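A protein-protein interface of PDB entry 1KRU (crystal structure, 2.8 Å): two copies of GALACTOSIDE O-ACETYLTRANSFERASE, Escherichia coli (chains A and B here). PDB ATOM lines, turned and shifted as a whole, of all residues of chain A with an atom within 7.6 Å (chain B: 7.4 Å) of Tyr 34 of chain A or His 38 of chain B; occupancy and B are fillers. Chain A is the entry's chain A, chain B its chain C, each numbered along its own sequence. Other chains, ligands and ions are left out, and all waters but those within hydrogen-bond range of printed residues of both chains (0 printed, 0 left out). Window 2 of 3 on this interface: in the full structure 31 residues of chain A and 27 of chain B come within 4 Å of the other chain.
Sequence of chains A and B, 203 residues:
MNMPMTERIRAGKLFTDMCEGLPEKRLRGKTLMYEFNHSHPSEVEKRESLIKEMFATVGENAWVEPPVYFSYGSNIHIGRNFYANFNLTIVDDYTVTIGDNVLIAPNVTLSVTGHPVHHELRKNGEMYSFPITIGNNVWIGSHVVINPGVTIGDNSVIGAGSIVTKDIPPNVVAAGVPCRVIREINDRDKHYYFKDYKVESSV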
ATOM      1  N   ARG A  28     -29.041 -23.971 -29.274  1.00  0.00           N
ATOM      2  CA  ARG A  28     -30.145 -24.310 -28.380  1.00  0.00           C
ATOM      3  C   ARG A  28     -29.702 -24.164 -26.929  1.00  0.00           C
ATOM      4  O   ARG A  28     -30.478 -23.741 -26.075  1.00  0.00           O
ATOM      5  CB  ARG A  28     -30.609 -25.753 -28.628  1.00  0.00           C
ATOM      6  CG  ARG A  28     -32.112 -25.978 -28.494  1.00  0.00           C
ATOM      7  CD  ARG A  28     -32.527 -27.349 -29.048  1.00  0.00           C
ATOM      8  NE  ARG A  28     -31.975 -27.613 -30.382  1.00  0.00           N
ATOM      9  CZ  ARG A  28     -31.396 -28.758 -30.747  1.00  0.00           C
ATOM     10  NH1 ARG A  28     -31.290 -29.759 -29.870  1.00  0.00           N
ATOM     11  NH2 ARG A  28     -30.918 -28.908 -31.985  1.00  0.00           N
ATOM     12  N   GLY A  29     -28.444 -24.504 -26.662  1.00  0.00           N
ATOM     13  CA  GLY A  29     -27.918 -24.433 -25.311  1.00  0.00           C
ATOM     14  C   GLY A  29     -27.506 -23.056 -24.843  1.00  0.00           C
ATOM     15  O   GLY A  29     -27.682 -22.708 -23.675  1.00  0.00           O
ATOM     16  N   LYS A  30     -26.936 -22.268 -25.743  1.00  0.00           N
ATOM     17  CA  LYS A  30     -26.534 -20.924 -25.380  1.00  0.00           C
ATOM     18  C   LYS A  30     -27.800 -20.092 -25.221  1.00  0.00           C
ATOM     19  O   LYS A  30     -27.796 -19.051 -24.560  1.00  0.00           O
ATOM     20  CB  LYS A  30     -25.601 -20.337 -26.450  1.00  0.00           C
ATOM     21  CG  LYS A  30     -24.313 -21.131 -26.630  1.00  0.00           C
ATOM     22  CD  LYS A  30     -23.110 -20.387 -26.087  1.00  0.00           C
ATOM     23  CE  LYS A  30     -21.871 -21.283 -26.006  1.00  0.00           C
ATOM     24  NZ  LYS A  30     -21.645 -22.125 -27.216  1.00  0.00           N
ATOM     25  N   THR A  31     -28.891 -20.563 -25.821  1.00  0.00           N
ATOM     26  CA  THR A  31     -30.173 -19.876 -25.726  1.00  0.00           C
ATOM     27  C   THR A  31     -30.744 -20.074 -24.332  1.00  0.00           C
ATOM     28  O   THR A  31     -31.204 -19.124 -23.694  1.00  0.00           O
ATOM     29  CB  THR A  31     -31.183 -20.412 -26.739  1.00  0.00           C
ATOM     30  OG1 THR A  31     -30.824 -19.957 -28.043  1.00  0.00           O
ATOM     31  CG2 THR A  31     -32.571 -19.917 -26.421  1.00  0.00           C
ATOM     32  N   LEU A  32     -30.709 -21.313 -23.854  1.00  0.00           N
ATOM     33  CA  LEU A  32     -31.221 -21.601 -22.524  1.00  0.00           C
ATOM     34  C   LEU A  32     -30.359 -20.934 -21.457  1.00  0.00           C
ATOM     35  O   LEU A  32     -30.860 -20.419 -20.457  1.00  0.00           O
ATOM     36  CB  LEU A  32     -31.260 -23.112 -22.290  1.00  0.00           C
ATOM     37  CG  LEU A  32     -32.542 -23.855 -22.669  1.00  0.00           C
ATOM     38  CD1 LEU A  32     -33.311 -23.093 -23.717  1.00  0.00           C
ATOM     39  CD2 LEU A  32     -32.169 -25.228 -23.193  1.00  0.00           C
ATOM     40  N   MET A  33     -29.055 -20.940 -21.697  1.00  0.00           N
ATOM     41  CA  MET A  33     -28.078 -20.371 -20.781  1.00  0.00           C
ATOM     42  C   MET A  33     -28.164 -18.847 -20.678  1.00  0.00           C
ATOM     43  O   MET A  33     -27.863 -18.273 -19.629  1.00  0.00           O
ATOM     44  CB  MET A  33     -26.678 -20.805 -21.221  1.00  0.00           C
ATOM     45  CG  MET A  33     -25.549 -19.914 -20.762  1.00  0.00           C
ATOM     46  SD  MET A  33     -24.057 -20.212 -21.736  1.00  0.00           S
ATOM     47  CE  MET A  33     -23.671 -18.595 -22.224  1.00  0.00           C
ATOM     48  N   TYR A  34     -28.574 -18.194 -21.759  1.00  0.00           N
ATOM     49  CA  TYR A  34     -28.695 -16.736 -21.760  1.00  0.00           C
ATOM     50  C   TYR A  34     -29.925 -16.331 -20.963  1.00  0.00           C
ATOM     51  O   TYR A  34     -29.994 -15.241 -20.416  1.00  0.00           O
ATOM     52  CB  TYR A  34     -28.790 -16.215 -23.202  1.00  0.00           C
ATOM     53  CG  TYR A  34     -29.339 -14.818 -23.313  1.00  0.00           C
ATOM     54  CD1 TYR A  34     -28.500 -13.703 -23.225  1.00  0.00           C
ATOM     55  CD2 TYR A  34     -30.700 -14.605 -23.495  1.00  0.00           C
ATOM     56  CE1 TYR A  34     -29.015 -12.400 -23.313  1.00  0.00           C
ATOM     57  CE2 TYR A  34     -31.227 -13.317 -23.584  1.00  0.00           C
ATOM     58  CZ  TYR A  34     -30.384 -12.219 -23.494  1.00  0.00           C
ATOM     59  OH  TYR A  34     -30.936 -10.959 -23.590  1.00  0.00           O
ATOM     60  N   GLU A  35     -30.899 -17.228 -20.916  1.00  0.00           N
ATOM     61  CA  GLU A  35     -32.137 -17.011 -20.177  1.00  0.00           C
ATOM     62  C   GLU A  35     -31.885 -17.218 -18.692  1.00  0.00           C
ATOM     63  O   GLU A  35     -32.511 -16.571 -17.860  1.00  0.00           O
ATOM     64  CB  GLU A  35     -33.216 -17.999 -20.628  1.00  0.00           C
ATOM     65  CG  GLU A  35     -33.669 -17.825 -22.052  1.00  0.00           C
ATOM     66  CD  GLU A  35     -35.008 -18.457 -22.304  1.00  0.00           C
ATOM     67  OE1 GLU A  35     -35.784 -18.620 -21.337  1.00  0.00           O
ATOM     68  OE2 GLU A  35     -35.280 -18.787 -23.474  1.00  0.00           O
ATOM     69  N   PHE A  36     -30.986 -18.140 -18.366  1.00  0.00           N
ATOM     70  CA  PHE A  36     -30.657 -18.430 -16.978  1.00  0.00           C
ATOM     71  C   PHE A  36     -29.822 -17.320 -16.357  1.00  0.00           C
ATOM     72  O   PHE A  36     -30.073 -16.894 -15.228  1.00  0.00           O
ATOM     73  CB  PHE A  36     -29.894 -19.756 -16.885  1.00  0.00           C
ATOM     74  CG  PHE A  36     -29.556 -20.176 -15.473  1.00  0.00           C
ATOM     75  CD1 PHE A  36     -30.519 -20.759 -14.653  1.00  0.00           C
ATOM     76  CD2 PHE A  36     -28.272 -20.008 -14.969  1.00  0.00           C
ATOM     77  CE1 PHE A  36     -30.203 -21.169 -13.348  1.00  0.00           C
ATOM     78  CE2 PHE A  36     -27.952 -20.416 -13.668  1.00  0.00           C
ATOM     79  CZ  PHE A  36     -28.919 -20.996 -12.858  1.00  0.00           C
ATOM     80  N   ASN A  37     -28.827 -16.862 -17.108  1.00  0.00           N
ATOM     81  CA  ASN A  37     -27.912 -15.822 -16.655  1.00  0.00           C
ATOM     82  C   ASN A  37     -28.516 -14.430 -16.560  1.00  0.00           C
ATOM     83  O   ASN A  37     -27.979 -13.566 -15.872  1.00  0.00           O
ATOM     84  CB  ASN A  37     -26.692 -15.783 -17.569  1.00  0.00           C
ATOM     85  CG  ASN A  37     -25.883 -17.067 -17.520  1.00  0.00           C
ATOM     86  OD1 ASN A  37     -25.130 -17.373 -18.450  1.00  0.00           O
ATOM     87  ND2 ASN A  37     -26.035 -17.825 -16.434  1.00  0.00           N
ATOM     88  N   HIS A  38     -29.629 -14.203 -17.252  1.00  0.00           N
ATOM     89  CA  HIS A  38     -30.276 -12.896 -17.227  1.00  0.00           C
ATOM     90  C   HIS A  38     -31.520 -12.915 -16.374  1.00  0.00           C
ATOM     91  O   HIS A  38     -32.181 -11.893 -16.189  1.00  0.00           O
ATOM     92  CB  HIS A  38     -30.636 -12.455 -18.641  1.00  0.00           C
ATOM     93  CG  HIS A  38     -29.458 -12.006 -19.439  1.00  0.00           C
ATOM     94  ND1 HIS A  38     -29.147 -10.675 -19.624  1.00  0.00           N
ATOM     95  CD2 HIS A  38     -28.480 -12.712 -20.052  1.00  0.00           C
ATOM     96  CE1 HIS A  38     -28.026 -10.584 -20.314  1.00  0.00           C
ATOM     97  NE2 HIS A  38     -27.600 -11.806 -20.587  1.00  0.00           N
ATOM     98  N   SER A  39     -31.830 -14.089 -15.844  1.00  0.00           N
ATOM     99  CA  SER A  39     -33.000 -14.254 -15.013  1.00  0.00           C
ATOM    100  C   SER A  39     -32.859 -13.487 -13.703  1.00  0.00           C
ATOM    101  O   SER A  39     -31.774 -13.405 -13.120  1.00  0.00           O
ATOM    102  CB  SER A  39     -33.224 -15.728 -14.732  1.00  0.00           C
ATOM    103  OG  SER A  39     -32.214 -16.206 -13.888  1.00  0.00           O
ATOM    104  N   LYS A  46     -38.394 -20.357 -12.129  1.00  0.00           N
ATOM    105  CA  LYS A  46     -37.889 -20.373 -13.495  1.00  0.00           C
ATOM    106  C   LYS A  46     -36.462 -20.925 -13.567  1.00  0.00           C
ATOM    107  O   LYS A  46     -36.115 -21.667 -14.495  1.00  0.00           O
ATOM    108  CB  LYS A  46     -37.926 -18.971 -14.092  1.00  0.00           C
ATOM    109  CG  LYS A  46     -37.529 -18.930 -15.553  1.00  0.00           C
ATOM    110  CD  LYS A  46     -37.417 -17.488 -16.033  1.00  0.00           C
ATOM    111  CE  LYS A  46     -35.962 -17.067 -16.266  1.00  0.00           C
ATOM    112  NZ  LYS A  46     -35.840 -15.763 -17.001  1.00  0.00           N
ATOM    113  N   LEU A  50     -35.111 -24.279 -15.230  1.00  0.00           N
ATOM    114  CA  LEU A  50     -34.198 -24.008 -16.330  1.00  0.00           C
ATOM    115  C   LEU A  50     -32.992 -24.919 -16.214  1.00  0.00           C
ATOM    116  O   LEU A  50     -32.488 -25.410 -17.225  1.00  0.00           O
ATOM    117  CB  LEU A  50     -33.744 -22.544 -16.331  1.00  0.00           C
ATOM    118  CG  LEU A  50     -34.434 -21.655 -17.370  1.00  0.00           C
ATOM    119  CD1 LEU A  50     -33.985 -20.223 -17.176  1.00  0.00           C
ATOM    120  CD2 LEU A  50     -34.104 -22.129 -18.759  1.00  0.00           C
ATOM    121  N   MET A  54     -31.424 -27.276 -19.121  1.00  0.00           N
ATOM    122  CA  MET A  54     -30.055 -27.053 -19.575  1.00  0.00           C
ATOM    123  C   MET A  54     -29.137 -28.267 -19.614  1.00  0.00           C
ATOM    124  O   MET A  54     -28.494 -28.521 -20.623  1.00  0.00           O
ATOM    125  CB  MET A  54     -29.379 -25.995 -18.707  1.00  0.00           C
ATOM    126  CG  MET A  54     -30.085 -24.676 -18.638  1.00  0.00           C
ATOM    127  SD  MET A  54     -29.059 -23.502 -17.728  1.00  0.00           S
ATOM    128  CE  MET A  54     -28.948 -24.243 -16.139  1.00  0.00           C
ATOM    129  N   VAL A  68     -23.622 -19.022 -15.398  1.00  0.00           N
ATOM    130  CA  VAL A  68     -23.004 -20.312 -15.672  1.00  0.00           C
ATOM    131  C   VAL A  68     -22.669 -20.302 -17.145  1.00  0.00           C
ATOM    132  O   VAL A  68     -23.424 -19.755 -17.939  1.00  0.00           O
ATOM    133  CB  VAL A  68     -23.969 -21.471 -15.442  1.00  0.00           C
ATOM    134  CG1 VAL A  68     -23.193 -22.764 -15.320  1.00  0.00           C
ATOM    135  CG2 VAL A  68     -24.780 -21.223 -14.209  1.00  0.00           C
ATOM    136  N   PHE A  70     -21.313 -22.737 -20.550  1.00  0.00           N
ATOM    137  CA  PHE A  70     -20.983 -24.031 -21.149  1.00  0.00           C
ATOM    138  C   PHE A  70     -21.115 -23.978 -22.659  1.00  0.00           C
ATOM    139  O   PHE A  70     -21.654 -23.009 -23.207  1.00  0.00           O
ATOM    140  CB  PHE A  70     -21.888 -25.145 -20.608  1.00  0.00           C
ATOM    141  CG  PHE A  70     -23.339 -24.772 -20.510  1.00  0.00           C
ATOM    142  CD1 PHE A  70     -23.908 -24.481 -19.274  1.00  0.00           C
ATOM    143  CD2 PHE A  70     -24.142 -24.720 -21.648  1.00  0.00           C
ATOM    144  CE1 PHE A  70     -25.251 -24.148 -19.177  1.00  0.00           C
ATOM    145  CE2 PHE A  70     -25.486 -24.387 -21.560  1.00  0.00           C
ATOM    146  CZ  PHE A  70     -26.042 -24.099 -20.323  1.00  0.00           C
ATOM    147  N   LEU B  32     -20.830  -0.022 -26.521  1.00  0.00           N
ATOM    148  CA  LEU B  32     -20.842  -1.059 -27.558  1.00  0.00           C
ATOM    149  C   LEU B  32     -20.683  -2.432 -26.913  1.00  0.00           C
ATOM    150  O   LEU B  32     -21.328  -3.410 -27.304  1.00  0.00           O
ATOM    151  CB  LEU B  32     -19.697  -0.840 -28.555  1.00  0.00           C
ATOM    152  CG  LEU B  32     -19.868  -0.100 -29.890  1.00  0.00           C
ATOM    153  CD1 LEU B  32     -21.206   0.605 -29.956  1.00  0.00           C
ATOM    154  CD2 LEU B  32     -18.720   0.900 -30.038  1.00  0.00           C
ATOM    155  N   MET B  33     -19.805  -2.490 -25.919  1.00  0.00           N
ATOM    156  CA  MET B  33     -19.536  -3.720 -25.196  1.00  0.00           C
ATOM    157  C   MET B  33     -20.801  -4.210 -24.504  1.00  0.00           C
ATOM    158  O   MET B  33     -21.157  -5.381 -24.627  1.00  0.00           O
ATOM    159  CB  MET B  33     -18.418  -3.475 -24.169  1.00  0.00           C
ATOM    160  CG  MET B  33     -18.471  -4.366 -22.940  1.00  0.00           C
ATOM    161  SD  MET B  33     -17.089  -4.035 -21.837  1.00  0.00           S
ATOM    162  CE  MET B  33     -17.912  -3.774 -20.301  1.00  0.00           C
ATOM    163  N   TYR B  34     -21.476  -3.311 -23.785  1.00  0.00           N
ATOM    164  CA  TYR B  34     -22.711  -3.646 -23.064  1.00  0.00           C
ATOM    165  C   TYR B  34     -23.731  -4.247 -24.026  1.00  0.00           C
ATOM    166  O   TYR B  34     -24.436  -5.197 -23.690  1.00  0.00           O
ATOM    167  CB  TYR B  34     -23.279  -2.393 -22.371  1.00  0.00           C
ATOM    168  CG  TYR B  34     -24.704  -2.520 -21.870  1.00  0.00           C
ATOM    169  CD1 TYR B  34     -24.980  -3.059 -20.610  1.00  0.00           C
ATOM    170  CD2 TYR B  34     -25.778  -2.111 -22.654  1.00  0.00           C
ATOM    171  CE1 TYR B  34     -26.299  -3.190 -20.143  1.00  0.00           C
ATOM    172  CE2 TYR B  34     -27.103  -2.238 -22.198  1.00  0.00           C
ATOM    173  CZ  TYR B  34     -27.356  -2.778 -20.944  1.00  0.00           C
ATOM    174  OH  TYR B  34     -28.663  -2.905 -20.511  1.00  0.00           O
ATOM    175  N   GLU B  35     -23.790  -3.698 -25.233  1.00  0.00           N
ATOM    176  CA  GLU B  35     -24.707  -4.198 -26.242  1.00  0.00           C
ATOM    177  C   GLU B  35     -24.353  -5.595 -26.696  1.00  0.00           C
ATOM    178  O   GLU B  35     -25.228  -6.432 -26.922  1.00  0.00           O
ATOM    179  CB  GLU B  35     -24.703  -3.284 -27.446  1.00  0.00           C
ATOM    180  CG  GLU B  35     -25.540  -2.070 -27.239  1.00  0.00           C
ATOM    181  CD  GLU B  35     -25.992  -1.482 -28.545  1.00  0.00           C
ATOM    182  OE1 GLU B  35     -26.786  -2.151 -29.249  1.00  0.00           O
ATOM    183  OE2 GLU B  35     -25.543  -0.358 -28.870  1.00  0.00           O
ATOM    184  N   PHE B  36     -23.061  -5.836 -26.843  1.00  0.00           N
ATOM    185  CA  PHE B  36     -22.587  -7.129 -27.277  1.00  0.00           C
ATOM    186  C   PHE B  36     -22.811  -8.203 -26.207  1.00  0.00           C
ATOM    187  O   PHE B  36     -23.235  -9.323 -26.500  1.00  0.00           O
ATOM    188  CB  PHE B  36     -21.107  -7.027 -27.640  1.00  0.00           C
ATOM    189  CG  PHE B  36     -20.535  -8.297 -28.163  1.00  0.00           C
ATOM    190  CD1 PHE B  36     -20.693  -8.644 -29.494  1.00  0.00           C
ATOM    191  CD2 PHE B  36     -19.883  -9.179 -27.310  1.00  0.00           C
ATOM    192  CE1 PHE B  36     -20.214  -9.851 -29.967  1.00  0.00           C
ATOM    193  CE2 PHE B  36     -19.403 -10.388 -27.774  1.00  0.00           C
ATOM    194  CZ  PHE B  36     -19.571 -10.727 -29.107  1.00  0.00           C
ATOM    195  N   ASN B  37     -22.536  -7.854 -24.960  1.00  0.00           N
ATOM    196  CA  ASN B  37     -22.701  -8.788 -23.864  1.00  0.00           C
ATOM    197  C   ASN B  37     -24.169  -9.104 -23.541  1.00  0.00           C
ATOM    198  O   ASN B  37     -24.470 -10.145 -22.947  1.00  0.00           O
ATOM    199  CB  ASN B  37     -21.997  -8.240 -22.622  1.00  0.00           C
ATOM    200  CG  ASN B  37     -20.478  -8.326 -22.721  1.00  0.00           C
ATOM    201  OD1 ASN B  37     -19.764  -7.678 -21.950  1.00  0.00           O
ATOM    202  ND2 ASN B  37     -19.977  -9.129 -23.665  1.00  0.00           N
ATOM    203  N   HIS B  38     -25.079  -8.214 -23.933  1.00  0.00           N
ATOM    204  CA  HIS B  38     -26.502  -8.412 -23.670  1.00  0.00           C
ATOM    205  C   HIS B  38     -27.291  -8.926 -24.856  1.00  0.00           C
ATOM    206  O   HIS B  38     -28.479  -9.211 -24.732  1.00  0.00           O
ATOM    207  CB  HIS B  38     -27.135  -7.117 -23.172  1.00  0.00           C
ATOM    208  CG  HIS B  38     -26.812  -6.815 -21.748  1.00  0.00           C
ATOM    209  ND1 HIS B  38     -27.578  -7.274 -20.701  1.00  0.00           N
ATOM    210  CD2 HIS B  38     -25.769  -6.161 -21.194  1.00  0.00           C
ATOM    211  CE1 HIS B  38     -27.016  -6.916 -19.559  1.00  0.00           C
ATOM    212  NE2 HIS B  38     -25.916  -6.239 -19.830  1.00  0.00           N
ATOM    213  N   SER B  39     -26.633  -9.052 -26.003  1.00  0.00           N
ATOM    214  CA  SER B  39     -27.296  -9.537 -27.211  1.00  0.00           C
ATOM    215  C   SER B  39     -27.729 -10.994 -27.058  1.00  0.00           C
ATOM    216  O   SER B  39     -27.144 -11.757 -26.287  1.00  0.00           O
ATOM    217  CB  SER B  39     -26.370  -9.398 -28.422  1.00  0.00           C
ATOM    218  OG  SER B  39     -25.211 -10.189 -28.259  1.00  0.00           O
ATOM    219  N   HIS B  40     -28.766 -11.373 -27.797  1.00  0.00           N
ATOM    220  CA  HIS B  40     -29.281 -12.729 -27.755  1.00  0.00           C
ATOM    221  C   HIS B  40     -28.398 -13.592 -28.627  1.00  0.00           C
ATOM    222  O   HIS B  40     -27.991 -13.174 -29.710  1.00  0.00           O
ATOM    223  CB  HIS B  40     -30.712 -12.777 -28.279  1.00  0.00           C
ATOM    224  CG  HIS B  40     -31.449 -14.026 -27.911  1.00  0.00           C
ATOM    225  ND1 HIS B  40     -31.430 -15.159 -28.693  1.00  0.00           N
ATOM    226  CD2 HIS B  40     -32.233 -14.313 -26.847  1.00  0.00           C
ATOM    227  CE1 HIS B  40     -32.177 -16.092 -28.124  1.00  0.00           C
ATOM    228  NE2 HIS B  40     -32.673 -15.602 -27.006  1.00  0.00           N
ATOM    229  N   PRO B  41     -28.112 -14.823 -28.177  1.00  0.00           N
ATOM    230  CA  PRO B  41     -27.262 -15.754 -28.924  1.00  0.00           C
ATOM    231  C   PRO B  41     -27.747 -15.948 -30.348  1.00  0.00           C
ATOM    232  O   PRO B  41     -27.015 -16.421 -31.213  1.00  0.00           O
ATOM    233  CB  PRO B  41     -27.335 -17.047 -28.109  1.00  0.00           C
ATOM    234  CG  PRO B  41     -28.462 -16.869 -27.169  1.00  0.00           C
ATOM    235  CD  PRO B  41     -28.611 -15.417 -26.925  1.00  0.00           C
ATOM    236  N   SER B  42     -28.990 -15.559 -30.583  1.00  0.00           N
ATOM    237  CA  SER B  42     -29.596 -15.691 -31.902  1.00  0.00           C
ATOM    238  C   SER B  42     -29.341 -14.487 -32.803  1.00  0.00           C
ATOM    239  O   SER B  42     -29.563 -14.561 -34.011  1.00  0.00           O
ATOM    240  CB  SER B  42     -31.106 -15.888 -31.767  1.00  0.00           C
ATOM    241  OG  SER B  42     -31.743 -14.641 -31.535  1.00  0.00           O
ATOM    242  N   GLU B  43     -28.899 -13.372 -32.228  1.00  0.00           N
ATOM    243  CA  GLU B  43     -28.640 -12.182 -33.027  1.00  0.00           C
ATOM    244  C   GLU B  43     -27.224 -12.218 -33.621  1.00  0.00           C
ATOM    245  O   GLU B  43     -26.426 -11.293 -33.461  1.00  0.00           O
ATOM    246  CB  GLU B  43     -28.861 -10.933 -32.169  1.00  0.00           C
ATOM    247  CG  GLU B  43     -30.250 -10.879 -31.563  1.00  0.00           C
ATOM    248  CD  GLU B  43     -30.420  -9.734 -30.587  1.00  0.00           C
ATOM    249  OE1 GLU B  43     -30.711  -9.988 -29.398  1.00  0.00           O
ATOM    250  OE2 GLU B  43     -30.262  -8.569 -31.004  1.00  0.00           O
ATOM    251  N   LYS B  46     -26.083  -9.100 -35.658  1.00  0.00           N
ATOM    252  CA  LYS B  46     -25.861  -7.907 -34.847  1.00  0.00           C
ATOM    253  C   LYS B  46     -24.529  -8.052 -34.113  1.00  0.00           C
ATOM    254  O   LYS B  46     -23.814  -7.074 -33.877  1.00  0.00           O
ATOM    255  CB  LYS B  46     -27.006  -7.753 -33.843  1.00  0.00           C
ATOM    256  CG  LYS B  46     -26.952  -6.500 -32.999  1.00  0.00           C
ATOM    257  CD  LYS B  46     -28.136  -6.436 -32.045  1.00  0.00           C
ATOM    258  CE  LYS B  46     -27.716  -6.856 -30.647  1.00  0.00           C
ATOM    259  NZ  LYS B  46     -28.696  -6.436 -29.601  1.00  0.00           N
ATOM    260  N   ARG B  47     -24.210  -9.295 -33.761  1.00  0.00           N
ATOM    261  CA  ARG B  47     -22.976  -9.615 -33.056  1.00  0.00           C
ATOM    262  C   ARG B  47     -21.783  -9.450 -33.987  1.00  0.00           C
ATOM    263  O   ARG B  47     -20.827  -8.751 -33.663  1.00  0.00           O
ATOM    264  CB  ARG B  47     -23.026 -11.054 -32.530  1.00  0.00           C
ATOM    265  CG  ARG B  47     -23.781 -11.222 -31.233  1.00  0.00           C
ATOM    266  CD  ARG B  47     -23.742 -12.660 -30.742  1.00  0.00           C
ATOM    267  NE  ARG B  47     -24.221 -12.737 -29.365  1.00  0.00           N
ATOM    268  CZ  ARG B  47     -24.198 -13.834 -28.613  1.00  0.00           C
ATOM    269  NH1 ARG B  47     -23.709 -14.971 -29.100  1.00  0.00           N
ATOM    270  NH2 ARG B  47     -24.664 -13.784 -27.371  1.00  0.00           N
ATOM    271  N   LEU B  50     -21.117  -6.005 -34.603  1.00  0.00           N
ATOM    272  CA  LEU B  50     -20.768  -5.286 -33.374  1.00  0.00           C
ATOM    273  C   LEU B  50     -19.272  -5.382 -33.066  1.00  0.00           C
ATOM    274  O   LEU B  50     -18.666  -4.429 -32.575  1.00  0.00           O
ATOM    275  CB  LEU B  50     -21.568  -5.836 -32.183  1.00  0.00           C
ATOM    276  CG  LEU B  50     -22.663  -4.946 -31.575  1.00  0.00           C
ATOM    277  CD1 LEU B  50     -23.572  -5.764 -30.666  1.00  0.00           C
ATOM    278  CD2 LEU B  50     -22.018  -3.834 -30.797  1.00  0.00           C
ATOM    279  N   PRO B  66     -19.547 -14.148 -25.989  1.00  0.00           N
ATOM    280  CA  PRO B  66     -19.826 -13.187 -24.909  1.00  0.00           C
ATOM    281  C   PRO B  66     -19.824 -13.921 -23.568  1.00  0.00           C
ATOM    282  O   PRO B  66     -20.160 -15.097 -23.512  1.00  0.00           O
ATOM    283  CB  PRO B  66     -21.219 -12.632 -25.244  1.00  0.00           C
ATOM    284  CG  PRO B  66     -21.514 -13.094 -26.619  1.00  0.00           C
ATOM    285  CD  PRO B  66     -20.717 -14.331 -26.862  1.00  0.00           C
ATOM    286  N   PRO B  67     -19.486 -13.223 -22.469  1.00  0.00           N
ATOM    287  CA  PRO B  67     -19.119 -11.808 -22.441  1.00  0.00           C
ATOM    288  C   PRO B  67     -17.646 -11.485 -22.655  1.00  0.00           C
ATOM    289  O   PRO B  67     -16.762 -12.298 -22.382  1.00  0.00           O
ATOM    290  CB  PRO B  67     -19.594 -11.351 -21.059  1.00  0.00           C
ATOM    291  CG  PRO B  67     -19.437 -12.569 -20.199  1.00  0.00           C
ATOM    292  CD  PRO B  67     -19.479 -13.795 -21.110  1.00  0.00           C
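The backbone carbonyl oxygen (O) of Phe 36 of chain B lies within hydrogen-bond range of the side-chain hydroxyl (OG) of Ser 39 of chain B. The guanidinium group (NE) of Arg 47 of chain B sits at hydrogen-bond distance from the side-chain hydroxyl (OG) of Ser 39 of chain B. The side-chain hydroxyl (OG) of Ser 42 of chain B lies within hydrogen-bond range of a ring nitrogen (ND1) of His 40 of chain B, at 2.9 Å. The backbone NH (N) of His 40 of chain B is in hydrogen-bond range of the side-chain carboxylate (OE1) of Glu 43 of chain B (2.9 Å).
Among the printed residues, pairs that only touch across the chains: Lys 30 of chain A with Pro 41 of chain B, Thr 31 of chain A with Pro 41 of chain B, Tyr 34 of chain A with Ser 39 of chain B, Tyr 34 of chain A with His 40 of chain B, Tyr 34 of chain A with Pro 41 of chain B and His 38 of chain A with His 38 of chain B.
Tyr 34 of chain A touches His 38 of chain B, but with the chains exchanged His 38 of chain A does not touch Tyr 34 of chain B (7.3 Å). Tyr 34 of chain A touches Ser 39 of chain B, but with the chains exchanged Ser 39 of chain A does not touch Tyr 34 of chain B (12.5 Å). His 38 of chain B touches its own counterpart, His 38 of chain A. Positions printed for both chains: 32, 33, 34, 35, 36, 37, 38, 39, 46 and 50. Of the 7 pairs that touch across the chains among the printed residues, 1 has its exchanged pair printed and touching as well.
The side-chain hydroxyl of Tyr 34 of chain A sits at hydrogen-bond distance from the backbone carbonyl oxygen of His 38 of chain B (3.2 Å).
Hydrophobic or aromatic side chains of chain A within 4 Å of the printed part of chain B: Tyr 34 and His 38. Of the 17 printed residues of chain B, 4 touch a printed residue of chain A. Printed residues of chain B that touch a printed residue of chain A: His 38, Ser 39, His 40 and Pro 41. Hydrophobic or aromatic side chains of chain B within 4 Å of the printed part of chain A: His 38, His 40 and Pro 41. Among the printed residues, no Asp or Glu carboxylate lies within 4 Å of a Lys or Arg side-chain nitrogen of the other chain.
Of the printed residues of chain B, Lys 30 of chain A touches Pro 41. Of the printed residues of chain B, Thr 31 of chain A touches Pro 41 (3.7 Å). Tyr 34 of chain A touches just these residues of chain B: His 38 (3.2 Å), Ser 39 (3.6 Å), His 40 (3.6 Å) and Pro 41 (3.7 Å). Glu 35 of chain A touches none of the printed residues of chain B. Printed residues of chain B within 4 Å of His 38 of chain A: His 38. Phe 70 of chain A touches none of the printed residues of chain B. His 38 of chain B touches two residues of chain A. Of the printed residues of chain A, His 40 of chain B touches Tyr 34 (3.6 Å). Of the printed residues of chain A, Pro 41 of chain B touches Lys 30 (3.5 Å), Thr 31 (3.7 Å) and Tyr 34 (3.7 Å). The nearest residue of chain B that does not touch Tyr 34 of chain A is Asn 37 of chain B (5.1 Å). The nearest printed residue of chain A that does not touch His 38 of chain B is Asn 37 of chain A (7.7 Å).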
